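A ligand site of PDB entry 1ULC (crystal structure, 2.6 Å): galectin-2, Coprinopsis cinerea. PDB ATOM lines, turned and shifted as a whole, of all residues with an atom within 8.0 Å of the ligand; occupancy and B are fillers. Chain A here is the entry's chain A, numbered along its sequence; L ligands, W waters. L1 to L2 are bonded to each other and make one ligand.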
ATOM      1  N   THR A  36      15.399  18.501 -30.799  1.00  0.00           N
ATOM      2  CA  THR A  36      15.852  19.519 -29.864  1.00  0.00           C
ATOM      3  C   THR A  36      15.113  20.834 -30.052  1.00  0.00           C
ATOM      4  O   THR A  36      15.039  21.373 -31.165  1.00  0.00           O
ATOM      5  CB  THR A  36      17.362  19.732 -29.985  1.00  0.00           C
ATOM      6  OG1 THR A  36      18.025  18.558 -29.491  1.00  0.00           O
ATOM      7  CG2 THR A  36      17.816  20.935 -29.178  1.00  0.00           C
ATOM      8  N   VAL A  38      14.726  24.753 -28.417  1.00  0.00           N
ATOM      9  CA  VAL A  38      15.402  25.756 -27.610  1.00  0.00           C
ATOM     10  C   VAL A  38      14.592  27.012 -27.322  1.00  0.00           C
ATOM     11  O   VAL A  38      13.813  27.465 -28.166  1.00  0.00           O
ATOM     12  CB  VAL A  38      16.737  26.181 -28.287  1.00  0.00           C
ATOM     13  CG1 VAL A  38      17.331  27.379 -27.579  1.00  0.00           C
ATOM     14  CG2 VAL A  38      17.710  25.021 -28.266  1.00  0.00           C
ATOM     15  N   ASN A  40      15.444  30.828 -25.554  1.00  0.00           N
ATOM     16  CA  ASN A  40      16.443  31.742 -24.990  1.00  0.00           C
ATOM     17  C   ASN A  40      15.840  33.022 -24.447  1.00  0.00           C
ATOM     18  O   ASN A  40      14.930  33.591 -25.048  1.00  0.00           O
ATOM     19  CB  ASN A  40      17.466  32.170 -26.056  1.00  0.00           C
ATOM     20  CG  ASN A  40      18.330  31.034 -26.529  1.00  0.00           C
ATOM     21  OD1 ASN A  40      18.849  30.253 -25.742  1.00  0.00           O
ATOM     22  ND2 ASN A  40      18.500  30.949 -27.841  1.00  0.00           N
ATOM     23  N   HIS A  51      19.575  30.011 -21.326  1.00  0.00           N
ATOM     24  CA  HIS A  51      19.442  29.124 -22.482  1.00  0.00           C
ATOM     25  C   HIS A  51      18.872  27.798 -21.995  1.00  0.00           C
ATOM     26  O   HIS A  51      19.414  27.184 -21.062  1.00  0.00           O
ATOM     27  CB  HIS A  51      20.816  28.881 -23.132  1.00  0.00           C
ATOM     28  CG  HIS A  51      20.822  27.838 -24.226  1.00  0.00           C
ATOM     29  ND1 HIS A  51      20.243  28.053 -25.457  1.00  0.00           N
ATOM     30  CD2 HIS A  51      21.355  26.598 -24.265  1.00  0.00           C
ATOM     31  CE1 HIS A  51      20.424  26.978 -26.213  1.00  0.00           C
ATOM     32  NE2 HIS A  51      21.088  26.085 -25.518  1.00  0.00           N
ATOM     33  N   ILE A  52      17.779  27.370 -22.607  1.00  0.00           N
ATOM     34  CA  ILE A  52      17.145  26.112 -22.261  1.00  0.00           C
ATOM     35  C   ILE A  52      17.155  25.248 -23.517  1.00  0.00           C
ATOM     36  O   ILE A  52      16.548  25.582 -24.529  1.00  0.00           O
ATOM     37  CB  ILE A  52      15.678  26.283 -21.813  1.00  0.00           C
ATOM     38  CG1 ILE A  52      15.577  27.380 -20.750  1.00  0.00           C
ATOM     39  CG2 ILE A  52      15.159  24.990 -21.228  1.00  0.00           C
ATOM     40  CD1 ILE A  52      14.142  27.656 -20.277  1.00  0.00           C
ATOM     41  N   SER A  53      17.873  24.133 -23.443  1.00  0.00           N
ATOM     42  CA  SER A  53      17.979  23.228 -24.568  1.00  0.00           C
ATOM     43  C   SER A  53      17.288  21.923 -24.178  1.00  0.00           C
ATOM     44  O   SER A  53      17.805  21.149 -23.370  1.00  0.00           O
ATOM     45  CB  SER A  53      19.443  22.978 -24.925  1.00  0.00           C
ATOM     46  OG  SER A  53      19.567  22.186 -26.090  1.00  0.00           O
ATOM     47  N   ILE A  54      16.109  21.703 -24.748  1.00  0.00           N
ATOM     48  CA  ILE A  54      15.316  20.503 -24.496  1.00  0.00           C
ATOM     49  C   ILE A  54      15.697  19.436 -25.530  1.00  0.00           C
ATOM     50  O   ILE A  54      15.296  19.508 -26.694  1.00  0.00           O
ATOM     51  CB  ILE A  54      13.822  20.829 -24.597  1.00  0.00           C
ATOM     52  CG1 ILE A  54      13.513  22.029 -23.719  1.00  0.00           C
ATOM     53  CG2 ILE A  54      12.991  19.636 -24.171  1.00  0.00           C
ATOM     54  CD1 ILE A  54      12.156  22.621 -23.975  1.00  0.00           C
ATOM     55  N   ARG A  55      16.475  18.457 -25.095  1.00  0.00           N
ATOM     56  CA  ARG A  55      16.941  17.399 -25.978  1.00  0.00           C
ATOM     57  C   ARG A  55      16.261  16.066 -25.701  1.00  0.00           C
ATOM     58  O   ARG A  55      16.660  15.324 -24.804  1.00  0.00           O
ATOM     59  CB  ARG A  55      18.450  17.248 -25.838  1.00  0.00           C
ATOM     60  CG  ARG A  55      19.172  18.563 -25.941  1.00  0.00           C
ATOM     61  CD  ARG A  55      20.612  18.454 -25.510  1.00  0.00           C
ATOM     62  NE  ARG A  55      21.285  19.743 -25.631  1.00  0.00           N
ATOM     63  CZ  ARG A  55      22.580  19.948 -25.419  1.00  0.00           C
ATOM     64  NH1 ARG A  55      23.366  18.934 -25.075  1.00  0.00           N
ATOM     65  NH2 ARG A  55      23.080  21.159 -25.559  1.00  0.00           N
ATOM     66  N   GLU A  58      18.375  12.727 -26.359  1.00  0.00           N
ATOM     67  CA  GLU A  58      19.597  12.616 -25.559  1.00  0.00           C
ATOM     68  C   GLU A  58      19.094  12.516 -24.126  1.00  0.00           C
ATOM     69  O   GLU A  58      19.868  12.402 -23.180  1.00  0.00           O
ATOM     70  CB  GLU A  58      20.410  13.901 -25.780  1.00  0.00           C
ATOM     71  CG  GLU A  58      21.916  13.827 -25.577  1.00  0.00           C
ATOM     72  CD  GLU A  58      22.606  15.161 -25.952  1.00  0.00           C
ATOM     73  OE1 GLU A  58      22.381  15.664 -27.081  1.00  0.00           O
ATOM     74  OE2 GLU A  58      23.390  15.691 -25.122  1.00  0.00           O
ATOM     75  N   VAL A  60      17.753  14.724 -22.066  1.00  0.00           N
ATOM     76  CA  VAL A  60      18.286  15.711 -21.152  1.00  0.00           C
ATOM     77  C   VAL A  60      17.866  17.120 -21.556  1.00  0.00           C
ATOM     78  O   VAL A  60      17.616  17.398 -22.731  1.00  0.00           O
ATOM     79  CB  VAL A  60      19.835  15.622 -21.087  1.00  0.00           C
ATOM     80  CG1 VAL A  60      20.444  16.071 -22.422  1.00  0.00           C
ATOM     81  CG2 VAL A  60      20.349  16.473 -19.941  1.00  0.00           C
ATOM     82  N   VAL A  62      19.271  20.956 -21.153  1.00  0.00           N
ATOM     83  CA  VAL A  62      20.491  21.664 -20.781  1.00  0.00           C
ATOM     84  C   VAL A  62      20.283  23.157 -20.565  1.00  0.00           C
ATOM     85  O   VAL A  62      19.639  23.816 -21.366  1.00  0.00           O
ATOM     86  CB  VAL A  62      21.589  21.487 -21.850  1.00  0.00           C
ATOM     87  CG1 VAL A  62      22.902  22.063 -21.356  1.00  0.00           C
ATOM     88  CG2 VAL A  62      21.742  20.019 -22.206  1.00  0.00           C
ATOM     89  N   PHE A  63      20.849  23.673 -19.481  1.00  0.00           N
ATOM     90  CA  PHE A  63      20.737  25.090 -19.156  1.00  0.00           C
ATOM     91  C   PHE A  63      22.121  25.725 -19.237  1.00  0.00           C
ATOM     92  O   PHE A  63      23.093  25.169 -18.743  1.00  0.00           O
ATOM     93  CB  PHE A  63      20.169  25.304 -17.741  1.00  0.00           C
ATOM     94  CG  PHE A  63      18.772  24.796 -17.575  1.00  0.00           C
ATOM     95  CD1 PHE A  63      18.529  23.445 -17.353  1.00  0.00           C
ATOM     96  CD2 PHE A  63      17.683  25.657 -17.674  1.00  0.00           C
ATOM     97  CE1 PHE A  63      17.227  22.954 -17.226  1.00  0.00           C
ATOM     98  CE2 PHE A  63      16.371  25.181 -17.548  1.00  0.00           C
ATOM     99  CZ  PHE A  63      16.148  23.829 -17.324  1.00  0.00           C
ATOM    100  N   ASN A  64      22.197  26.890 -19.876  1.00  0.00           N
ATOM    101  CA  ASN A  64      23.471  27.587 -20.025  1.00  0.00           C
ATOM    102  C   ASN A  64      23.246  29.065 -20.345  1.00  0.00           C
ATOM    103  O   ASN A  64      22.114  29.526 -20.486  1.00  0.00           O
ATOM    104  CB  ASN A  64      24.301  26.941 -21.139  1.00  0.00           C
ATOM    105  CG  ASN A  64      25.801  26.973 -20.843  1.00  0.00           C
ATOM    106  OD1 ASN A  64      26.278  27.836 -20.120  1.00  0.00           O
ATOM    107  ND2 ASN A  64      26.544  26.027 -21.427  1.00  0.00           N
ATOM    108  N   SER A  65      24.356  29.805 -20.446  1.00  0.00           N
ATOM    109  CA  SER A  65      24.348  31.231 -20.744  1.00  0.00           C
ATOM    110  C   SER A  65      25.584  31.541 -21.582  1.00  0.00           C
ATOM    111  O   SER A  65      26.528  30.751 -21.604  1.00  0.00           O
ATOM    112  CB  SER A  65      24.413  32.064 -19.452  1.00  0.00           C
ATOM    113  OG  SER A  65      23.311  31.847 -18.600  1.00  0.00           O
ATOM    114  N   ARG A  66      25.582  32.688 -22.250  1.00  0.00           N
ATOM    115  CA  ARG A  66      26.737  33.129 -23.024  1.00  0.00           C
ATOM    116  C   ARG A  66      26.453  34.513 -23.592  1.00  0.00           C
ATOM    117  O   ARG A  66      25.307  34.855 -23.856  1.00  0.00           O
ATOM    118  CB  ARG A  66      27.090  32.142 -24.153  1.00  0.00           C
ATOM    119  CG  ARG A  66      26.302  32.303 -25.427  1.00  0.00           C
ATOM    120  CD  ARG A  66      26.780  31.317 -26.493  1.00  0.00           C
ATOM    121  NE  ARG A  66      26.104  31.537 -27.762  1.00  0.00           N
ATOM    122  CZ  ARG A  66      26.416  32.474 -28.641  1.00  0.00           C
ATOM    123  NH1 ARG A  66      27.425  33.306 -28.405  1.00  0.00           N
ATOM    124  NH2 ARG A  66      25.731  32.608 -29.756  1.00  0.00           N
ATOM    125  N   ALA A  71      31.717  32.433 -25.490  1.00  0.00           N
ATOM    126  CA  ALA A  71      31.591  30.987 -25.462  1.00  0.00           C
ATOM    127  C   ALA A  71      30.579  30.580 -24.403  1.00  0.00           C
ATOM    128  O   ALA A  71      30.213  31.372 -23.533  1.00  0.00           O
ATOM    129  CB  ALA A  71      32.931  30.353 -25.166  1.00  0.00           C
ATOM    130  N   TRP A  72      30.113  29.334 -24.509  1.00  0.00           N
ATOM    131  CA  TRP A  72      29.156  28.791 -23.551  1.00  0.00           C
ATOM    132  C   TRP A  72      29.899  28.576 -22.254  1.00  0.00           C
ATOM    133  O   TRP A  72      31.120  28.438 -22.243  1.00  0.00           O
ATOM    134  CB  TRP A  72      28.612  27.446 -24.028  1.00  0.00           C
ATOM    135  CG  TRP A  72      27.690  27.527 -25.202  1.00  0.00           C
ATOM    136  CD1 TRP A  72      27.919  27.064 -26.461  1.00  0.00           C
ATOM    137  CD2 TRP A  72      26.366  28.079 -25.206  1.00  0.00           C
ATOM    138  NE1 TRP A  72      26.823  27.282 -27.261  1.00  0.00           N
ATOM    139  CE2 TRP A  72      25.857  27.903 -26.510  1.00  0.00           C
ATOM    140  CE3 TRP A  72      25.569  28.690 -24.239  1.00  0.00           C
ATOM    141  CZ2 TRP A  72      24.565  28.323 -26.875  1.00  0.00           C
ATOM    142  CZ3 TRP A  72      24.286  29.103 -24.595  1.00  0.00           C
ATOM    143  CH2 TRP A  72      23.808  28.918 -25.903  1.00  0.00           C
ATOM    144  N   GLY A  73      29.162  28.553 -21.149  1.00  0.00           N
ATOM    145  CA  GLY A  73      29.774  28.307 -19.859  1.00  0.00           C
ATOM    146  C   GLY A  73      29.544  26.855 -19.508  1.00  0.00           C
ATOM    147  O   GLY A  73      29.325  26.025 -20.388  1.00  0.00           O
ATOM    148  N   PRO A  74      29.608  26.499 -18.224  1.00  0.00           N
ATOM    149  CA  PRO A  74      29.374  25.090 -17.916  1.00  0.00           C
ATOM    150  C   PRO A  74      27.880  24.744 -18.014  1.00  0.00           C
ATOM    151  O   PRO A  74      27.017  25.570 -17.685  1.00  0.00           O
ATOM    152  CB  PRO A  74      29.947  24.944 -16.500  1.00  0.00           C
ATOM    153  CG  PRO A  74      29.787  26.324 -15.918  1.00  0.00           C
ATOM    154  CD  PRO A  74      30.146  27.228 -17.069  1.00  0.00           C
ATOM    155  N   GLU A  75      27.563  23.538 -18.488  1.00  0.00           N
ATOM    156  CA  GLU A  75      26.172  23.132 -18.633  1.00  0.00           C
ATOM    157  C   GLU A  75      25.575  22.585 -17.354  1.00  0.00           C
ATOM    158  O   GLU A  75      26.222  21.848 -16.618  1.00  0.00           O
ATOM    159  CB  GLU A  75      26.034  22.053 -19.713  1.00  0.00           C
ATOM    160  CG  GLU A  75      26.494  22.458 -21.085  1.00  0.00           C
ATOM    161  CD  GLU A  75      26.144  21.430 -22.144  1.00  0.00           C
ATOM    162  OE1 GLU A  75      26.025  20.235 -21.788  1.00  0.00           O
ATOM    163  OE2 GLU A  75      26.010  21.810 -23.328  1.00  0.00           O
ATOM    164  N   GLU A  76      24.329  22.975 -17.110  1.00  0.00           N
ATOM    165  CA  GLU A  76      23.577  22.492 -15.960  1.00  0.00           C
ATOM    166  C   GLU A  76      22.480  21.654 -16.618  1.00  0.00           C
ATOM    167  O   GLU A  76      21.655  22.172 -17.375  1.00  0.00           O
ATOM    168  CB  GLU A  76      23.023  23.675 -15.149  1.00  0.00           C
ATOM    169  CG  GLU A  76      24.099  24.385 -14.352  1.00  0.00           C
ATOM    170  CD  GLU A  76      23.579  25.537 -13.495  1.00  0.00           C
ATOM    171  OE1 GLU A  76      22.547  25.376 -12.820  1.00  0.00           O
ATOM    172  OE2 GLU A  76      24.219  26.600 -13.494  1.00  0.00           O
ATOM    173  N   ARG A  77      22.497  20.355 -16.348  1.00  0.00           N
ATOM    174  CA  ARG A  77      21.553  19.418 -16.969  1.00  0.00           C
ATOM    175  C   ARG A  77      20.543  18.751 -16.032  1.00  0.00           C
ATOM    176  O   ARG A  77      20.654  18.839 -14.819  1.00  0.00           O
ATOM    177  CB  ARG A  77      22.351  18.309 -17.670  1.00  0.00           C
ATOM    178  CG  ARG A  77      23.269  18.770 -18.774  1.00  0.00           C
ATOM    179  CD  ARG A  77      24.422  17.789 -18.961  1.00  0.00           C
ATOM    180  NE  ARG A  77      25.074  17.945 -20.258  1.00  0.00           N
ATOM    181  CZ  ARG A  77      24.716  17.300 -21.358  1.00  0.00           C
ATOM    182  NH1 ARG A  77      23.709  16.436 -21.324  1.00  0.00           N
ATOM    183  NH2 ARG A  77      25.355  17.511 -22.499  1.00  0.00           N
ATOM    184  N   ARG A 115      24.039  34.487 -14.357  1.00  0.00           N
ATOM    185  CA  ARG A 115      25.465  34.579 -14.686  1.00  0.00           C
ATOM    186  C   ARG A 115      25.793  35.903 -15.355  1.00  0.00           C
ATOM    187  O   ARG A 115      26.932  36.370 -15.271  1.00  0.00           O
ATOM    188  CB  ARG A 115      25.862  33.425 -15.620  1.00  0.00           C
ATOM    189  CG  ARG A 115      25.641  32.034 -15.033  1.00  0.00           C
ATOM    190  CD  ARG A 115      26.134  30.976 -15.985  1.00  0.00           C
ATOM    191  NE  ARG A 115      25.875  29.630 -15.501  1.00  0.00           N
ATOM    192  CZ  ARG A 115      26.252  28.516 -16.124  1.00  0.00           C
ATOM    193  NH1 ARG A 115      26.905  28.579 -17.272  1.00  0.00           N
ATOM    194  NH2 ARG A 115      25.955  27.327 -15.600  1.00  0.00           N
HETATM  195  C1  LIG L   1      28.300  19.114 -25.230  1.00  0.00           C
HETATM  196  C2  LIG L   1      26.984  19.629 -25.816  1.00  0.00           C
HETATM  197  C3  LIG L   1      27.235  20.971 -26.521  1.00  0.00           C
HETATM  198  C4  LIG L   1      28.361  20.835 -27.558  1.00  0.00           C
HETATM  199  C5  LIG L   1      28.780  22.175 -28.125  1.00  0.00           C
HETATM  200  C6  LIG L   1      29.295  18.985 -26.365  1.00  0.00           C
HETATM  201  O1  LIG L   1      30.502  18.503 -25.875  1.00  0.00           O
HETATM  202  O2  LIG L   1      28.099  17.870 -24.590  1.00  0.00           O
HETATM  203  O3  LIG L   1      26.020  19.787 -24.791  1.00  0.00           O
HETATM  204  O4  LIG L   1      26.022  21.391 -27.175  1.00  0.00           O
HETATM  205  O5  LIG L   1      29.542  20.269 -26.943  1.00  0.00           O
HETATM  206  O6  LIG L   1      29.196  23.059 -27.088  1.00  0.00           O
HETATM  207  C1  LG2 L   2      25.750  22.747 -27.180  1.00  0.00           C
HETATM  208  C2  LG2 L   2      24.605  22.998 -28.170  1.00  0.00           C
HETATM  209  C3  LG2 L   2      24.105  24.441 -28.077  1.00  0.00           C
HETATM  210  C4  LG2 L   2      23.781  24.800 -26.622  1.00  0.00           C
HETATM  211  C5  LG2 L   2      24.986  24.506 -25.740  1.00  0.00           C
HETATM  212  C6  LG2 L   2      24.688  24.764 -24.284  1.00  0.00           C
HETATM  213  O1  LG2 L   2      25.060  22.724 -29.490  1.00  0.00           O
HETATM  214  O2  LG2 L   2      22.947  24.606 -28.884  1.00  0.00           O
HETATM  215  O3  LG2 L   2      22.666  24.050 -26.173  1.00  0.00           O
HETATM  216  O4  LG2 L   2      25.359  23.118 -25.853  1.00  0.00           O
HETATM  217  O5  LG2 L   2      25.823  24.530 -23.479  1.00  0.00           O
HETATM  218  O   HOH W   1      20.995  22.737 -28.407  1.00  0.00           O
HETATM  219  O   HOH W   2      31.624  16.857 -28.010  1.00  0.00           O
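NH2 of Arg 77 lies within hydrogen-bond range of O3 of LIG L1 (3.3 Å). NH1 of Arg 55 lies within hydrogen-bond range of O3 of LIG L1 (2.8 Å). An oxygen (O3) of LG2 L2 lies within hydrogen-bond range of a ring nitrogen (NE2) of His 51, at 2.7 Å. ND2 of Asn 64 lies within hydrogen-bond range of O5 of LG2 L2. An oxygen (O3) of LIG L1 lies within hydrogen-bond range of the side-chain carboxylate (OE2) of Glu 75.
ND1 of His 51 sits at hydrogen-bond distance from OD1 of Asn 40 (2.6 Å). The side-chain carboxylate (OE2) of Glu 58 lies within salt-bridge range of the guanidinium group (NH2) of Arg 77 (3.7 Å). The backbone carbonyl oxygen of Gly 73 sits at hydrogen-bond distance from the side-chain amide nitrogen of Asn 64, at 3.0 Å. O of Asn 64 is in hydrogen-bond range of N of His 51 (2.7 Å). O of Pro 74 lies close to OD1 of Asn 64. The backbone carbonyl oxygen of Val 60 lies within hydrogen-bond range of the backbone NH of Arg 55 (2.8 Å). O of Ser 53 is in hydrogen-bond range of N of Val 62 (2.7 Å). The side-chain carboxylate (OE2) of Glu 58 is in salt-bridge range of the guanidinium group (NH1) of Arg 55.
Merely in contact with the ligand: Trp 72 and Ser 53. Hydrophobic or aromatic side chains within 4 Å of the ligand: His 51 and Trp 72. Within 4 Å of the ligand: His 51, Ser 53, Arg 55, Asn 64, Trp 72, Glu 75 and Arg 77. The nearest printed residue that does not touch the ligand is Val 62 (4.4 Å).
Water W1 lies within hydrogen-bond range of an oxygen (O2) of LG2 L2 and the side-chain hydroxyl (OG) of Ser 53.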
